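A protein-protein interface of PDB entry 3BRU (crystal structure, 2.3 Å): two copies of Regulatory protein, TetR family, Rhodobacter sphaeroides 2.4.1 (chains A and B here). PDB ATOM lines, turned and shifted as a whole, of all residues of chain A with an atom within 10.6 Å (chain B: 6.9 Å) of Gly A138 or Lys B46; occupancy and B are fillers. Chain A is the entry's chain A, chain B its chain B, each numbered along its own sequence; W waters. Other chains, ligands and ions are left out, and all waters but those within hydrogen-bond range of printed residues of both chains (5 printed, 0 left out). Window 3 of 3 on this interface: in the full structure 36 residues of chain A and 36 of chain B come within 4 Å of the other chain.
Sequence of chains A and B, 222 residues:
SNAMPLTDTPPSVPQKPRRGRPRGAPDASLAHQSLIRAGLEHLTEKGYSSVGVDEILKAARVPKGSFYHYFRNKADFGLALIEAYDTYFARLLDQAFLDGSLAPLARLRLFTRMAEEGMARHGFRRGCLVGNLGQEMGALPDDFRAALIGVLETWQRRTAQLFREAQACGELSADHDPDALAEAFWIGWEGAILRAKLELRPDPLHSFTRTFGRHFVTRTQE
The side-chain hydroxyl of Ser B49 sits at hydrogen-bond distance from the side-chain hydroxyl of Ser A50, 3.0 Å away.
The side-chain hydroxyl (OG) of Ser B50 lies within hydrogen-bond range of the side-chain hydroxyl (OG) of Ser A49, 3.3 Å away.
OE1 of Gln A135 sits at hydrogen-bond distance from NZ of Lys B197 (2.8 Å).
NH2 of Arg A145 sits at hydrogen-bond distance from O of Lys B197.
OD1 of Asn B132 lies close to OE1 of Gln A135, 3.4 Å away.
N of Ser B49 sits at hydrogen-bond distance from OE2 of Glu B136 (2.9 Å).
The guanidinium group of Arg B125 is in salt-bridge range of the side-chain carboxylate of Glu B45.
The side-chain hydroxyl of Ser A49 lies within hydrogen-bond range of the side-chain carboxylate of Glu A136, at 2.9 Å.
The backbone carbonyl oxygen (O) of Leu B43 sits at hydrogen-bond distance from the side-chain amide nitrogen (ND2) of Asn B132 (2.8 Å).
ND2 of Asn B132 is in hydrogen-bond range of O of Thr B44 (2.9 Å).
NZ of Lys B46 lies within salt-bridge range of OE1 of Glu B55 (3.7 Å).
Among the printed residues, merely in contact across the chains: Ala A139 with Ser B50 (3.3 Å), Gly A138 with Glu B45 (3.5 Å), Ser A49 with Ser B49 (3.8 Å) and Gly A138 with Lys B46 (3.9 Å).
Gly A47 touches none of the printed residues of chain B.
Printed residues of chain B within 4 Å of Ser A49: Ser B49 (3.8 Å) and Ser B50 (3.3 Å).
Of the printed residues of chain B, Ser A50 touches Ser B49.
Gly A138 touches just these residues of chain B: Glu B45 (3.5 Å) and Lys B46 (3.9 Å).
Printed residues of chain B within 4 Å of Ala A139: Ser B50 (3.3 Å).
Glu B45 touches just one residue of chain A: Gly A138.
Lys B46 touches just one residue of chain A: Gly A138 (3.9 Å).
The nearest residue of chain B that does not touch Gly A138 is Lys B197 (5.3 Å).
The nearest residue of chain A that does not touch Lys B46 is Glu A136 (4.1 Å).
Printed residues of chain B that touch a printed residue of chain A: Glu B45, Lys B46, Ser B49, Ser B50, Asn B132 and Lys B197.
Printed residues of chain A that touch a printed residue of chain B: Ser A49, Ser A50, Gln A135, Gly A138, Ala A139 and Arg A145.
Hydrophobic or aromatic side chains of chain A within 4 Å of the printed part of chain B: Ala A139.
Along chain A the printed residues that touch a printed residue of chain B span positions 49 to 145.
Ser A49 touches its own counterpart, Ser B49.
Ser A49 touches Ser B50, and with the chains exchanged Ser A50 touches Ser B49.
6 positions are printed for both chains.
Of the 9 pairs that touch across the chains among the printed residues, 3 have their exchanged pair printed and touching as well.
Water W5 bridges OD1 of Asn B132 and OE1 of Gln A135.
Water W3 lies within hydrogen-bond range of the backbone carbonyl oxygen (O) of Lys B197 (2.8 Å) and the guanidinium group (NH2) of Arg A145 (3.0 Å).
Water W2 lies within hydrogen-bond range of the backbone carbonyl oxygen of Gln A135 (2.8 Å), the backbone carbonyl oxygen of Glu B45 (2.8 Å), the backbone NH of Gly A138 (2.9 Å) and the backbone NH of Met A137 (3.4 Å).
Water W1 lies within hydrogen-bond range of O of Gly A134 (2.9 Å) and NZ of Lys B197 (2.9 Å).
Water W4 lies within hydrogen-bond range of OE2 of Glu A136 (3.3 Å), OG of Ser B49 (3.3 Å) and OG of Ser A50 (3.3 Å).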
ATOM      1  N   GLY A  47      18.534   9.908  32.994  1.00  0.00           N
ATOM      2  CA  GLY A  47      18.173   8.565  32.618  1.00  0.00           C
ATOM      3  C   GLY A  47      19.180   8.156  31.571  1.00  0.00           C
ATOM      4  O   GLY A  47      20.106   8.922  31.247  1.00  0.00           O
ATOM      5  N   TYR A  48      19.000   6.955  31.033  1.00  0.00           N
ATOM      6  CA  TYR A  48      19.903   6.409  30.031  1.00  0.00           C
ATOM      7  C   TYR A  48      19.953   7.221  28.726  1.00  0.00           C
ATOM      8  O   TYR A  48      21.054   7.582  28.286  1.00  0.00           O
ATOM      9  CB  TYR A  48      19.518   4.964  29.779  1.00  0.00           C
ATOM     10  CG  TYR A  48      20.362   4.220  28.796  1.00  0.00           C
ATOM     11  CD1 TYR A  48      21.390   3.398  29.241  1.00  0.00           C
ATOM     12  CD2 TYR A  48      20.124   4.310  27.408  1.00  0.00           C
ATOM     13  CE1 TYR A  48      22.159   2.666  28.338  1.00  0.00           C
ATOM     14  CE2 TYR A  48      20.892   3.566  26.496  1.00  0.00           C
ATOM     15  CZ  TYR A  48      21.900   2.742  26.982  1.00  0.00           C
ATOM     16  OH  TYR A  48      22.705   2.018  26.145  1.00  0.00           O
ATOM     17  N   SER A  49      18.787   7.521  28.134  1.00  0.00           N
ATOM     18  CA  SER A  49      18.706   8.307  26.876  1.00  0.00           C
ATOM     19  C   SER A  49      19.355   9.702  26.925  1.00  0.00           C
ATOM     20  O   SER A  49      19.745  10.227  25.898  1.00  0.00           O
ATOM     21  CB  SER A  49      17.255   8.495  26.391  1.00  0.00           C
ATOM     22  OG  SER A  49      16.475   7.318  26.492  1.00  0.00           O
ATOM     23  N   SER A  50      19.443  10.288  28.125  1.00  0.00           N
ATOM     24  CA  SER A  50      19.933  11.649  28.351  1.00  0.00           C
ATOM     25  C   SER A  50      21.438  11.720  28.547  1.00  0.00           C
ATOM     26  O   SER A  50      22.049  12.783  28.471  1.00  0.00           O
ATOM     27  CB  SER A  50      19.295  12.186  29.627  1.00  0.00           C
ATOM     28  OG  SER A  50      18.289  13.109  29.296  1.00  0.00           O
ATOM     29  N   GLY A 131      13.304   2.137  37.961  1.00  0.00           N
ATOM     30  CA  GLY A 131      12.117   2.866  37.533  1.00  0.00           C
ATOM     31  C   GLY A 131      12.454   3.798  36.399  1.00  0.00           C
ATOM     32  O   GLY A 131      11.702   3.853  35.409  1.00  0.00           O
ATOM     33  N   ASN A 132      13.555   4.549  36.532  1.00  0.00           N
ATOM     34  CA  ASN A 132      13.981   5.440  35.425  1.00  0.00           C
ATOM     35  C   ASN A 132      14.158   4.682  34.121  1.00  0.00           C
ATOM     36  O   ASN A 132      13.669   5.126  33.088  1.00  0.00           O
ATOM     37  CB  ASN A 132      15.289   6.179  35.705  1.00  0.00           C
ATOM     38  CG  ASN A 132      15.180   7.219  36.816  1.00  0.00           C
ATOM     39  OD1 ASN A 132      14.135   7.383  37.486  1.00  0.00           O
ATOM     40  ND2 ASN A 132      16.276   7.942  37.019  1.00  0.00           N
ATOM     41  N   LEU A 133      14.877   3.560  34.146  1.00  0.00           N
ATOM     42  CA  LEU A 133      15.148   2.846  32.911  1.00  0.00           C
ATOM     43  C   LEU A 133      13.889   2.133  32.410  1.00  0.00           C
ATOM     44  O   LEU A 133      13.646   2.067  31.184  1.00  0.00           O
ATOM     45  CB  LEU A 133      16.287   1.844  33.072  1.00  0.00           C
ATOM     46  CG  LEU A 133      17.693   2.318  33.441  1.00  0.00           C
ATOM     47  CD1 LEU A 133      18.650   1.138  33.433  1.00  0.00           C
ATOM     48  CD2 LEU A 133      18.210   3.394  32.534  1.00  0.00           C
ATOM     49  N   GLY A 134      13.106   1.594  33.346  1.00  0.00           N
ATOM     50  CA  GLY A 134      11.842   0.922  33.023  1.00  0.00           C
ATOM     51  C   GLY A 134      10.879   1.778  32.214  1.00  0.00           C
ATOM     52  O   GLY A 134      10.318   1.338  31.202  1.00  0.00           O
ATOM     53  N   GLN A 135      10.683   3.003  32.675  1.00  0.00           N
ATOM     54  CA  GLN A 135       9.918   3.996  31.945  1.00  0.00           C
ATOM     55  C   GLN A 135      10.442   4.321  30.538  1.00  0.00           C
ATOM     56  O   GLN A 135       9.638   4.579  29.644  1.00  0.00           O
ATOM     57  CB  GLN A 135       9.787   5.284  32.762  1.00  0.00           C
ATOM     58  CG  GLN A 135       8.693   6.208  32.259  1.00  0.00           C
ATOM     59  CD  GLN A 135       7.269   5.698  32.541  1.00  0.00           C
ATOM     60  OE1 GLN A 135       6.876   4.633  32.064  1.00  0.00           O
ATOM     61  NE2 GLN A 135       6.476   6.498  33.273  1.00  0.00           N
ATOM     62  N   GLU A 136      11.758   4.334  30.327  1.00  0.00           N
ATOM     63  CA  GLU A 136      12.258   4.610  28.971  1.00  0.00           C
ATOM     64  C   GLU A 136      12.562   3.375  28.108  1.00  0.00           C
ATOM     65  O   GLU A 136      13.285   3.463  27.117  1.00  0.00           O
ATOM     66  CB  GLU A 136      13.450   5.574  28.998  1.00  0.00           C
ATOM     67  CG  GLU A 136      14.683   5.040  29.675  1.00  0.00           C
ATOM     68  CD  GLU A 136      15.646   6.171  30.103  1.00  0.00           C
ATOM     69  OE1 GLU A 136      16.137   6.082  31.277  1.00  0.00           O
ATOM     70  OE2 GLU A 136      15.890   7.132  29.283  1.00  0.00           O
ATOM     71  N   MET A 137      11.995   2.234  28.485  1.00  0.00           N
ATOM     72  CA  MET A 137      12.202   0.974  27.795  1.00  0.00           C
ATOM     73  C   MET A 137      12.089   1.062  26.246  1.00  0.00           C
ATOM     74  O   MET A 137      12.847   0.398  25.552  1.00  0.00           O
ATOM     75  CB  MET A 137      11.266  -0.096  28.375  1.00  0.00           C
ATOM     76  CG  MET A 137      11.556  -1.533  27.888  1.00  0.00           C
ATOM     77  SD  MET A 137      13.349  -2.244  28.254  1.00  0.00           S
ATOM     78  CE  MET A 137      13.980  -2.697  26.410  1.00  0.00           C
ATOM     79  N   GLY A 138      11.179   1.880  25.703  1.00  0.00           N
ATOM     80  CA  GLY A 138      11.065   2.018  24.252  1.00  0.00           C
ATOM     81  C   GLY A 138      12.363   2.477  23.569  1.00  0.00           C
ATOM     82  O   GLY A 138      12.564   2.209  22.372  1.00  0.00           O
ATOM     83  N   ALA A 139      13.251   3.160  24.308  1.00  0.00           N
ATOM     84  CA  ALA A 139      14.488   3.679  23.714  1.00  0.00           C
ATOM     85  C   ALA A 139      15.740   2.851  24.077  1.00  0.00           C
ATOM     86  O   ALA A 139      16.865   3.225  23.711  1.00  0.00           O
ATOM     87  CB  ALA A 139      14.681   5.157  24.068  1.00  0.00           C
ATOM     88  N   LEU A 140      15.532   1.724  24.766  1.00  0.00           N
ATOM     89  CA  LEU A 140      16.614   0.889  25.273  1.00  0.00           C
ATOM     90  C   LEU A 140      16.848  -0.332  24.402  1.00  0.00           C
ATOM     91  O   LEU A 140      15.919  -0.821  23.783  1.00  0.00           O
ATOM     92  CB  LEU A 140      16.314   0.434  26.716  1.00  0.00           C
ATOM     93  CG  LEU A 140      16.259   1.557  27.760  1.00  0.00           C
ATOM     94  CD1 LEU A 140      16.072   0.933  29.147  1.00  0.00           C
ATOM     95  CD2 LEU A 140      17.486   2.532  27.724  1.00  0.00           C
ATOM     96  N   PRO A 141      18.094  -0.846  24.387  1.00  0.00           N
ATOM     97  CA  PRO A 141      18.434  -2.138  23.739  1.00  0.00           C
ATOM     98  C   PRO A 141      17.555  -3.239  24.327  1.00  0.00           C
ATOM     99  O   PRO A 141      17.281  -3.195  25.526  1.00  0.00           O
ATOM    100  CB  PRO A 141      19.892  -2.380  24.174  1.00  0.00           C
ATOM    101  CG  PRO A 141      20.430  -1.025  24.538  1.00  0.00           C
ATOM    102  CD  PRO A 141      19.264  -0.228  25.057  1.00  0.00           C
ATOM    103  N   ASP A 142      17.100  -4.213  23.547  1.00  0.00           N
ATOM    104  CA  ASP A 142      16.139  -5.167  24.150  1.00  0.00           C
ATOM    105  C   ASP A 142      16.626  -6.098  25.286  1.00  0.00           C
ATOM    106  O   ASP A 142      15.799  -6.600  26.036  1.00  0.00           O
ATOM    107  CB  ASP A 142      15.220  -5.858  23.136  1.00  0.00           C
ATOM    108  CG  ASP A 142      13.783  -5.198  23.095  1.00  0.00           C
ATOM    109  OD1 ASP A 142      13.608  -4.127  22.434  1.00  0.00           O
ATOM    110  OD2 ASP A 142      12.825  -5.746  23.731  1.00  0.00           O
ATOM    111  N   ASP A 143      17.943  -6.262  25.440  1.00  0.00           N
ATOM    112  CA  ASP A 143      18.573  -6.918  26.627  1.00  0.00           C
ATOM    113  C   ASP A 143      18.076  -6.408  27.997  1.00  0.00           C
ATOM    114  O   ASP A 143      17.964  -7.160  28.967  1.00  0.00           O
ATOM    115  CB  ASP A 143      20.090  -6.682  26.598  1.00  0.00           C
ATOM    116  CG  ASP A 143      20.856  -7.834  25.973  1.00  0.00           C
ATOM    117  OD1 ASP A 143      20.217  -8.701  25.340  1.00  0.00           O
ATOM    118  OD2 ASP A 143      22.106  -7.888  26.113  1.00  0.00           O
ATOM    119  N   PHE A 144      17.812  -5.106  28.052  1.00  0.00           N
ATOM    120  CA  PHE A 144      17.421  -4.422  29.263  1.00  0.00           C
ATOM    121  C   PHE A 144      16.080  -4.925  29.821  1.00  0.00           C
ATOM    122  O   PHE A 144      15.937  -4.998  31.036  1.00  0.00           O
ATOM    123  CB  PHE A 144      17.377  -2.915  29.002  1.00  0.00           C
ATOM    124  CG  PHE A 144      18.736  -2.276  28.916  1.00  0.00           C
ATOM    125  CD1 PHE A 144      19.669  -2.691  27.969  1.00  0.00           C
ATOM    126  CD2 PHE A 144      19.094  -1.259  29.774  1.00  0.00           C
ATOM    127  CE1 PHE A 144      20.942  -2.093  27.904  1.00  0.00           C
ATOM    128  CE2 PHE A 144      20.354  -0.652  29.692  1.00  0.00           C
ATOM    129  CZ  PHE A 144      21.264  -1.067  28.748  1.00  0.00           C
ATOM    130  N   ARG A 145      15.129  -5.290  28.954  1.00  0.00           N
ATOM    131  CA  ARG A 145      13.808  -5.715  29.394  1.00  0.00           C
ATOM    132  C   ARG A 145      13.857  -6.816  30.484  1.00  0.00           C
ATOM    133  O   ARG A 145      13.344  -6.622  31.600  1.00  0.00           O
ATOM    134  CB  ARG A 145      12.919  -6.117  28.200  1.00  0.00           C
ATOM    135  CG  ARG A 145      11.404  -6.036  28.485  1.00  0.00           C
ATOM    136  CD  ARG A 145      10.481  -6.321  27.226  1.00  0.00           C
ATOM    137  NE  ARG A 145      10.717  -5.380  26.112  1.00  0.00           N
ATOM    138  CZ  ARG A 145      10.255  -4.127  26.060  1.00  0.00           C
ATOM    139  NH1 ARG A 145      10.544  -3.326  25.028  1.00  0.00           N
ATOM    140  NH2 ARG A 145       9.506  -3.653  27.039  1.00  0.00           N
ATOM    141  N   LEU A 148      15.786  -5.649  33.667  1.00  0.00           N
ATOM    142  CA  LEU A 148      14.978  -4.777  34.536  1.00  0.00           C
ATOM    143  C   LEU A 148      13.850  -5.542  35.236  1.00  0.00           C
ATOM    144  O   LEU A 148      13.634  -5.370  36.441  1.00  0.00           O
ATOM    145  CB  LEU A 148      14.425  -3.576  33.790  1.00  0.00           C
ATOM    146  CG  LEU A 148      15.421  -2.546  33.256  1.00  0.00           C
ATOM    147  CD1 LEU A 148      14.627  -1.693  32.235  1.00  0.00           C
ATOM    148  CD2 LEU A 148      16.109  -1.699  34.439  1.00  0.00           C
ATOM    149  N   GLU B  41       2.971  10.163  19.434  1.00  0.00           N
ATOM    150  CA  GLU B  41       3.403   8.758  19.235  1.00  0.00           C
ATOM    151  C   GLU B  41       4.829   8.484  19.761  1.00  0.00           C
ATOM    152  O   GLU B  41       5.096   7.464  20.430  1.00  0.00           O
ATOM    153  CB  GLU B  41       3.260   8.359  17.764  1.00  0.00           C
ATOM    154  CG  GLU B  41       1.800   8.360  17.330  1.00  0.00           C
ATOM    155  CD  GLU B  41       1.579   8.081  15.847  1.00  0.00           C
ATOM    156  OE1 GLU B  41       2.578   7.855  15.127  1.00  0.00           O
ATOM    157  OE2 GLU B  41       0.400   8.107  15.399  1.00  0.00           O
ATOM    158  N   HIS B  42       5.741   9.399  19.463  1.00  0.00           N
ATOM    159  CA  HIS B  42       7.094   9.251  19.891  1.00  0.00           C
ATOM    160  C   HIS B  42       7.280   9.499  21.387  1.00  0.00           C
ATOM    161  O   HIS B  42       8.035   8.763  22.041  1.00  0.00           O
ATOM    162  CB  HIS B  42       8.010  10.138  19.049  1.00  0.00           C
ATOM    163  CG  HIS B  42       8.185   9.642  17.648  1.00  0.00           C
ATOM    164  ND1 HIS B  42       7.161   9.641  16.721  1.00  0.00           N
ATOM    165  CD2 HIS B  42       9.257   9.096  17.024  1.00  0.00           C
ATOM    166  CE1 HIS B  42       7.597   9.131  15.584  1.00  0.00           C
ATOM    167  NE2 HIS B  42       8.868   8.801  15.736  1.00  0.00           N
ATOM    168  N   LEU B  43       6.606  10.492  21.953  1.00  0.00           N
ATOM    169  CA  LEU B  43       6.752  10.720  23.405  1.00  0.00           C
ATOM    170  C   LEU B  43       6.019   9.698  24.328  1.00  0.00           C
ATOM    171  O   LEU B  43       6.466   9.455  25.483  1.00  0.00           O
ATOM    172  CB  LEU B  43       6.407  12.168  23.807  1.00  0.00           C
ATOM    173  CG  LEU B  43       7.181  13.442  23.354  1.00  0.00           C
ATOM    174  CD1 LEU B  43       7.136  14.558  24.406  1.00  0.00           C
ATOM    175  CD2 LEU B  43       8.617  13.182  22.973  1.00  0.00           C
ATOM    176  N   THR B  44       4.891   9.137  23.870  1.00  0.00           N
ATOM    177  CA  THR B  44       4.259   8.039  24.631  1.00  0.00           C
ATOM    178  C   THR B  44       5.041   6.706  24.546  1.00  0.00           C
ATOM    179  O   THR B  44       5.007   5.877  25.448  1.00  0.00           O
ATOM    180  CB  THR B  44       2.814   7.822  24.235  1.00  0.00           C
ATOM    181  OG1 THR B  44       2.733   7.555  22.831  1.00  0.00           O
ATOM    182  CG2 THR B  44       1.943   9.070  24.607  1.00  0.00           C
ATOM    183  N   GLU B  45       5.776   6.530  23.469  1.00  0.00           N
ATOM    184  CA  GLU B  45       6.496   5.304  23.253  1.00  0.00           C
ATOM    185  C   GLU B  45       7.932   5.330  23.776  1.00  0.00           C
ATOM    186  O   GLU B  45       8.417   4.328  24.306  1.00  0.00           O
ATOM    187  CB  GLU B  45       6.501   4.968  21.773  1.00  0.00           C
ATOM    188  CG  GLU B  45       7.278   3.731  21.485  1.00  0.00           C
ATOM    189  CD  GLU B  45       6.981   3.184  20.130  1.00  0.00           C
ATOM    190  OE1 GLU B  45       6.350   3.919  19.324  1.00  0.00           O
ATOM    191  OE2 GLU B  45       7.372   2.015  19.877  1.00  0.00           O
ATOM    192  N   LYS B  46       8.623   6.448  23.586  1.00  0.00           N
ATOM    193  CA  LYS B  46      10.007   6.563  24.051  1.00  0.00           C
ATOM    194  C   LYS B  46      10.153   7.561  25.176  1.00  0.00           C
ATOM    195  O   LYS B  46      10.518   7.190  26.298  1.00  0.00           O
ATOM    196  CB  LYS B  46      10.951   6.897  22.895  1.00  0.00           C
ATOM    197  CG  LYS B  46      11.041   5.791  21.891  1.00  0.00           C
ATOM    198  CD  LYS B  46      11.415   6.321  20.556  1.00  0.00           C
ATOM    199  CE  LYS B  46      12.154   5.265  19.747  1.00  0.00           C
ATOM    200  NZ  LYS B  46      12.662   5.888  18.462  1.00  0.00           N
ATOM    201  N   GLY B  47       9.848   8.815  24.887  1.00  0.00           N
ATOM    202  CA  GLY B  47      10.044   9.924  25.800  1.00  0.00           C
ATOM    203  C   GLY B  47      10.740  11.042  25.047  1.00  0.00           C
ATOM    204  O   GLY B  47      11.147  10.875  23.913  1.00  0.00           O
ATOM    205  N   TYR B  48      10.905  12.178  25.698  1.00  0.00           N
ATOM    206  CA  TYR B  48      11.445  13.388  25.094  1.00  0.00           C
ATOM    207  C   TYR B  48      12.921  13.285  24.775  1.00  0.00           C
ATOM    208  O   TYR B  48      13.355  13.726  23.713  1.00  0.00           O
ATOM    209  CB  TYR B  48      11.205  14.505  26.089  1.00  0.00           C
ATOM    210  CG  TYR B  48      11.610  15.895  25.716  1.00  0.00           C
ATOM    211  CD1 TYR B  48      10.741  16.720  25.008  1.00  0.00           C
ATOM    212  CD2 TYR B  48      12.830  16.418  26.142  1.00  0.00           C
ATOM    213  CE1 TYR B  48      11.095  18.042  24.699  1.00  0.00           C
ATOM    214  CE2 TYR B  48      13.188  17.729  25.865  1.00  0.00           C
ATOM    215  CZ  TYR B  48      12.318  18.544  25.136  1.00  0.00           C
ATOM    216  OH  TYR B  48      12.667  19.860  24.831  1.00  0.00           O
ATOM    217  N   SER B  49      13.695  12.707  25.692  1.00  0.00           N
ATOM    218  CA  SER B  49      15.174  12.656  25.559  1.00  0.00           C
ATOM    219  C   SER B  49      15.688  11.931  24.310  1.00  0.00           C
ATOM    220  O   SER B  49      16.716  12.315  23.752  1.00  0.00           O
ATOM    221  CB  SER B  49      15.818  12.031  26.799  1.00  0.00           C
ATOM    222  OG  SER B  49      15.665  12.894  27.893  1.00  0.00           O
ATOM    223  N   SER B  50      14.955  10.898  23.896  1.00  0.00           N
ATOM    224  CA  SER B  50      15.275  10.025  22.757  1.00  0.00           C
ATOM    225  C   SER B  50      14.952  10.571  21.369  1.00  0.00           C
ATOM    226  O   SER B  50      15.383   9.976  20.390  1.00  0.00           O
ATOM    227  CB  SER B  50      14.513   8.709  22.909  1.00  0.00           C
ATOM    228  OG  SER B  50      14.331   8.400  24.288  1.00  0.00           O
ATOM    229  N   VAL B  51      14.194  11.660  21.275  1.00  0.00           N
ATOM    230  CA  VAL B  51      13.614  12.072  19.995  1.00  0.00           C
ATOM    231  C   VAL B  51      13.991  13.506  19.551  1.00  0.00           C
ATOM    232  O   VAL B  51      13.731  14.473  20.255  1.00  0.00           O
ATOM    233  CB  VAL B  51      12.018  11.924  19.962  1.00  0.00           C
ATOM    234  CG1 VAL B  51      11.495  10.424  20.389  1.00  0.00           C
ATOM    235  CG2 VAL B  51      11.343  13.096  20.751  1.00  0.00           C
ATOM    236  N   GLU B  55      13.732  13.169  13.464  1.00  0.00           N
ATOM    237  CA  GLU B  55      12.906  11.940  13.566  1.00  0.00           C
ATOM    238  C   GLU B  55      11.455  12.274  13.388  1.00  0.00           C
ATOM    239  O   GLU B  55      10.736  11.586  12.702  1.00  0.00           O
ATOM    240  CB  GLU B  55      12.966  11.311  14.949  1.00  0.00           C
ATOM    241  CG  GLU B  55      14.136  10.480  15.247  1.00  0.00           C
ATOM    242  CD  GLU B  55      14.142  10.042  16.714  1.00  0.00           C
ATOM    243  OE1 GLU B  55      13.162   9.364  17.152  1.00  0.00           O
ATOM    244  OE2 GLU B  55      15.136  10.379  17.414  1.00  0.00           O
ATOM    245  N   ARG B 125       3.074  -0.803  23.676  1.00  0.00           N
ATOM    246  CA  ARG B 125       4.269   0.002  23.416  1.00  0.00           C
ATOM    247  C   ARG B 125       4.160   1.464  23.830  1.00  0.00           C
ATOM    248  O   ARG B 125       5.187   2.121  24.051  1.00  0.00           O
ATOM    249  CB  ARG B 125       4.645  -0.109  21.946  1.00  0.00           C
ATOM    250  CG  ARG B 125       5.416  -1.374  21.683  1.00  0.00           C
ATOM    251  CD  ARG B 125       5.487  -1.767  20.242  1.00  0.00           C
ATOM    252  NE  ARG B 125       4.785  -0.859  19.333  1.00  0.00           N
ATOM    253  CZ  ARG B 125       3.787  -1.224  18.518  1.00  0.00           C
ATOM    254  NH1 ARG B 125       3.231  -0.303  17.714  1.00  0.00           N
ATOM    255  NH2 ARG B 125       3.348  -2.496  18.489  1.00  0.00           N
ATOM    256  N   ARG B 126       2.927   1.971  23.951  1.00  0.00           N
ATOM    257  CA  ARG B 126       2.706   3.373  24.262  1.00  0.00           C
ATOM    258  C   ARG B 126       2.027   3.576  25.616  1.00  0.00           C
ATOM    259  O   ARG B 126       0.965   2.988  25.874  1.00  0.00           O
ATOM    260  CB  ARG B 126       1.896   4.045  23.153  1.00  0.00           C
ATOM    261  CG  ARG B 126       2.558   3.976  21.790  1.00  0.00           C
ATOM    262  CD  ARG B 126       1.634   4.596  20.721  1.00  0.00           C
ATOM    263  NE  ARG B 126       2.082   4.236  19.375  1.00  0.00           N
ATOM    264  CZ  ARG B 126       1.471   4.578  18.239  1.00  0.00           C
ATOM    265  NH1 ARG B 126       0.371   5.332  18.250  1.00  0.00           N
ATOM    266  NH2 ARG B 126       1.987   4.171  17.083  1.00  0.00           N
ATOM    267  N   ASN B 132       5.808   9.418  31.326  1.00  0.00           N
ATOM    268  CA  ASN B 132       7.091   9.407  30.621  1.00  0.00           C
ATOM    269  C   ASN B 132       7.934  10.665  30.849  1.00  0.00           C
ATOM    270  O   ASN B 132       9.126  10.558  31.236  1.00  0.00           O
ATOM    271  CB  ASN B 132       6.929   9.177  29.125  1.00  0.00           C
ATOM    272  CG  ASN B 132       6.444   7.750  28.785  1.00  0.00           C
ATOM    273  OD1 ASN B 132       6.154   6.939  29.675  1.00  0.00           O
ATOM    274  ND2 ASN B 132       6.336   7.452  27.480  1.00  0.00           N
ATOM    275  N   GLU B 136      11.463  11.502  33.331  1.00  0.00           N
ATOM    276  CA  GLU B 136      12.668  12.178  32.807  1.00  0.00           C
ATOM    277  C   GLU B 136      12.887  13.573  33.353  1.00  0.00           C
ATOM    278  O   GLU B 136      13.787  14.258  32.875  1.00  0.00           O
ATOM    279  CB  GLU B 136      12.603  12.368  31.287  1.00  0.00           C
ATOM    280  CG  GLU B 136      12.540  11.137  30.480  1.00  0.00           C
ATOM    281  CD  GLU B 136      12.072  11.399  29.039  1.00  0.00           C
ATOM    282  OE1 GLU B 136      10.870  11.702  28.808  1.00  0.00           O
ATOM    283  OE2 GLU B 136      12.916  11.245  28.122  1.00  0.00           O
ATOM    284  N   LYS B 197       3.979  -1.168  29.983  1.00  0.00           N
ATOM    285  CA  LYS B 197       4.824  -0.797  28.850  1.00  0.00           C
ATOM    286  C   LYS B 197       6.176  -1.507  28.914  1.00  0.00           C
ATOM    287  O   LYS B 197       6.762  -1.834  27.897  1.00  0.00           O
ATOM    288  CB  LYS B 197       5.001   0.727  28.839  1.00  0.00           C
ATOM    289  CG  LYS B 197       5.791   1.273  27.664  1.00  0.00           C
ATOM    290  CD  LYS B 197       5.559   2.772  27.484  1.00  0.00           C
ATOM    291  CE  LYS B 197       6.741   3.565  27.987  1.00  0.00           C
ATOM    292  NZ  LYS B 197       6.559   3.853  29.403  1.00  0.00           N
HETATM  293  O   HOH W   1       7.485   1.375  30.619  1.00  0.00           O
HETATM  294  O   HOH W   2       9.379   3.789  26.926  1.00  0.00           O
HETATM  295  O   HOH W   3       8.614  -0.987  25.983  1.00  0.00           O
HETATM  296  O   HOH W   4      16.537  10.328  29.776  1.00  0.00           O
HETATM  297  O   HOH W   5       3.866   5.838  30.840  1.00  0.00           O
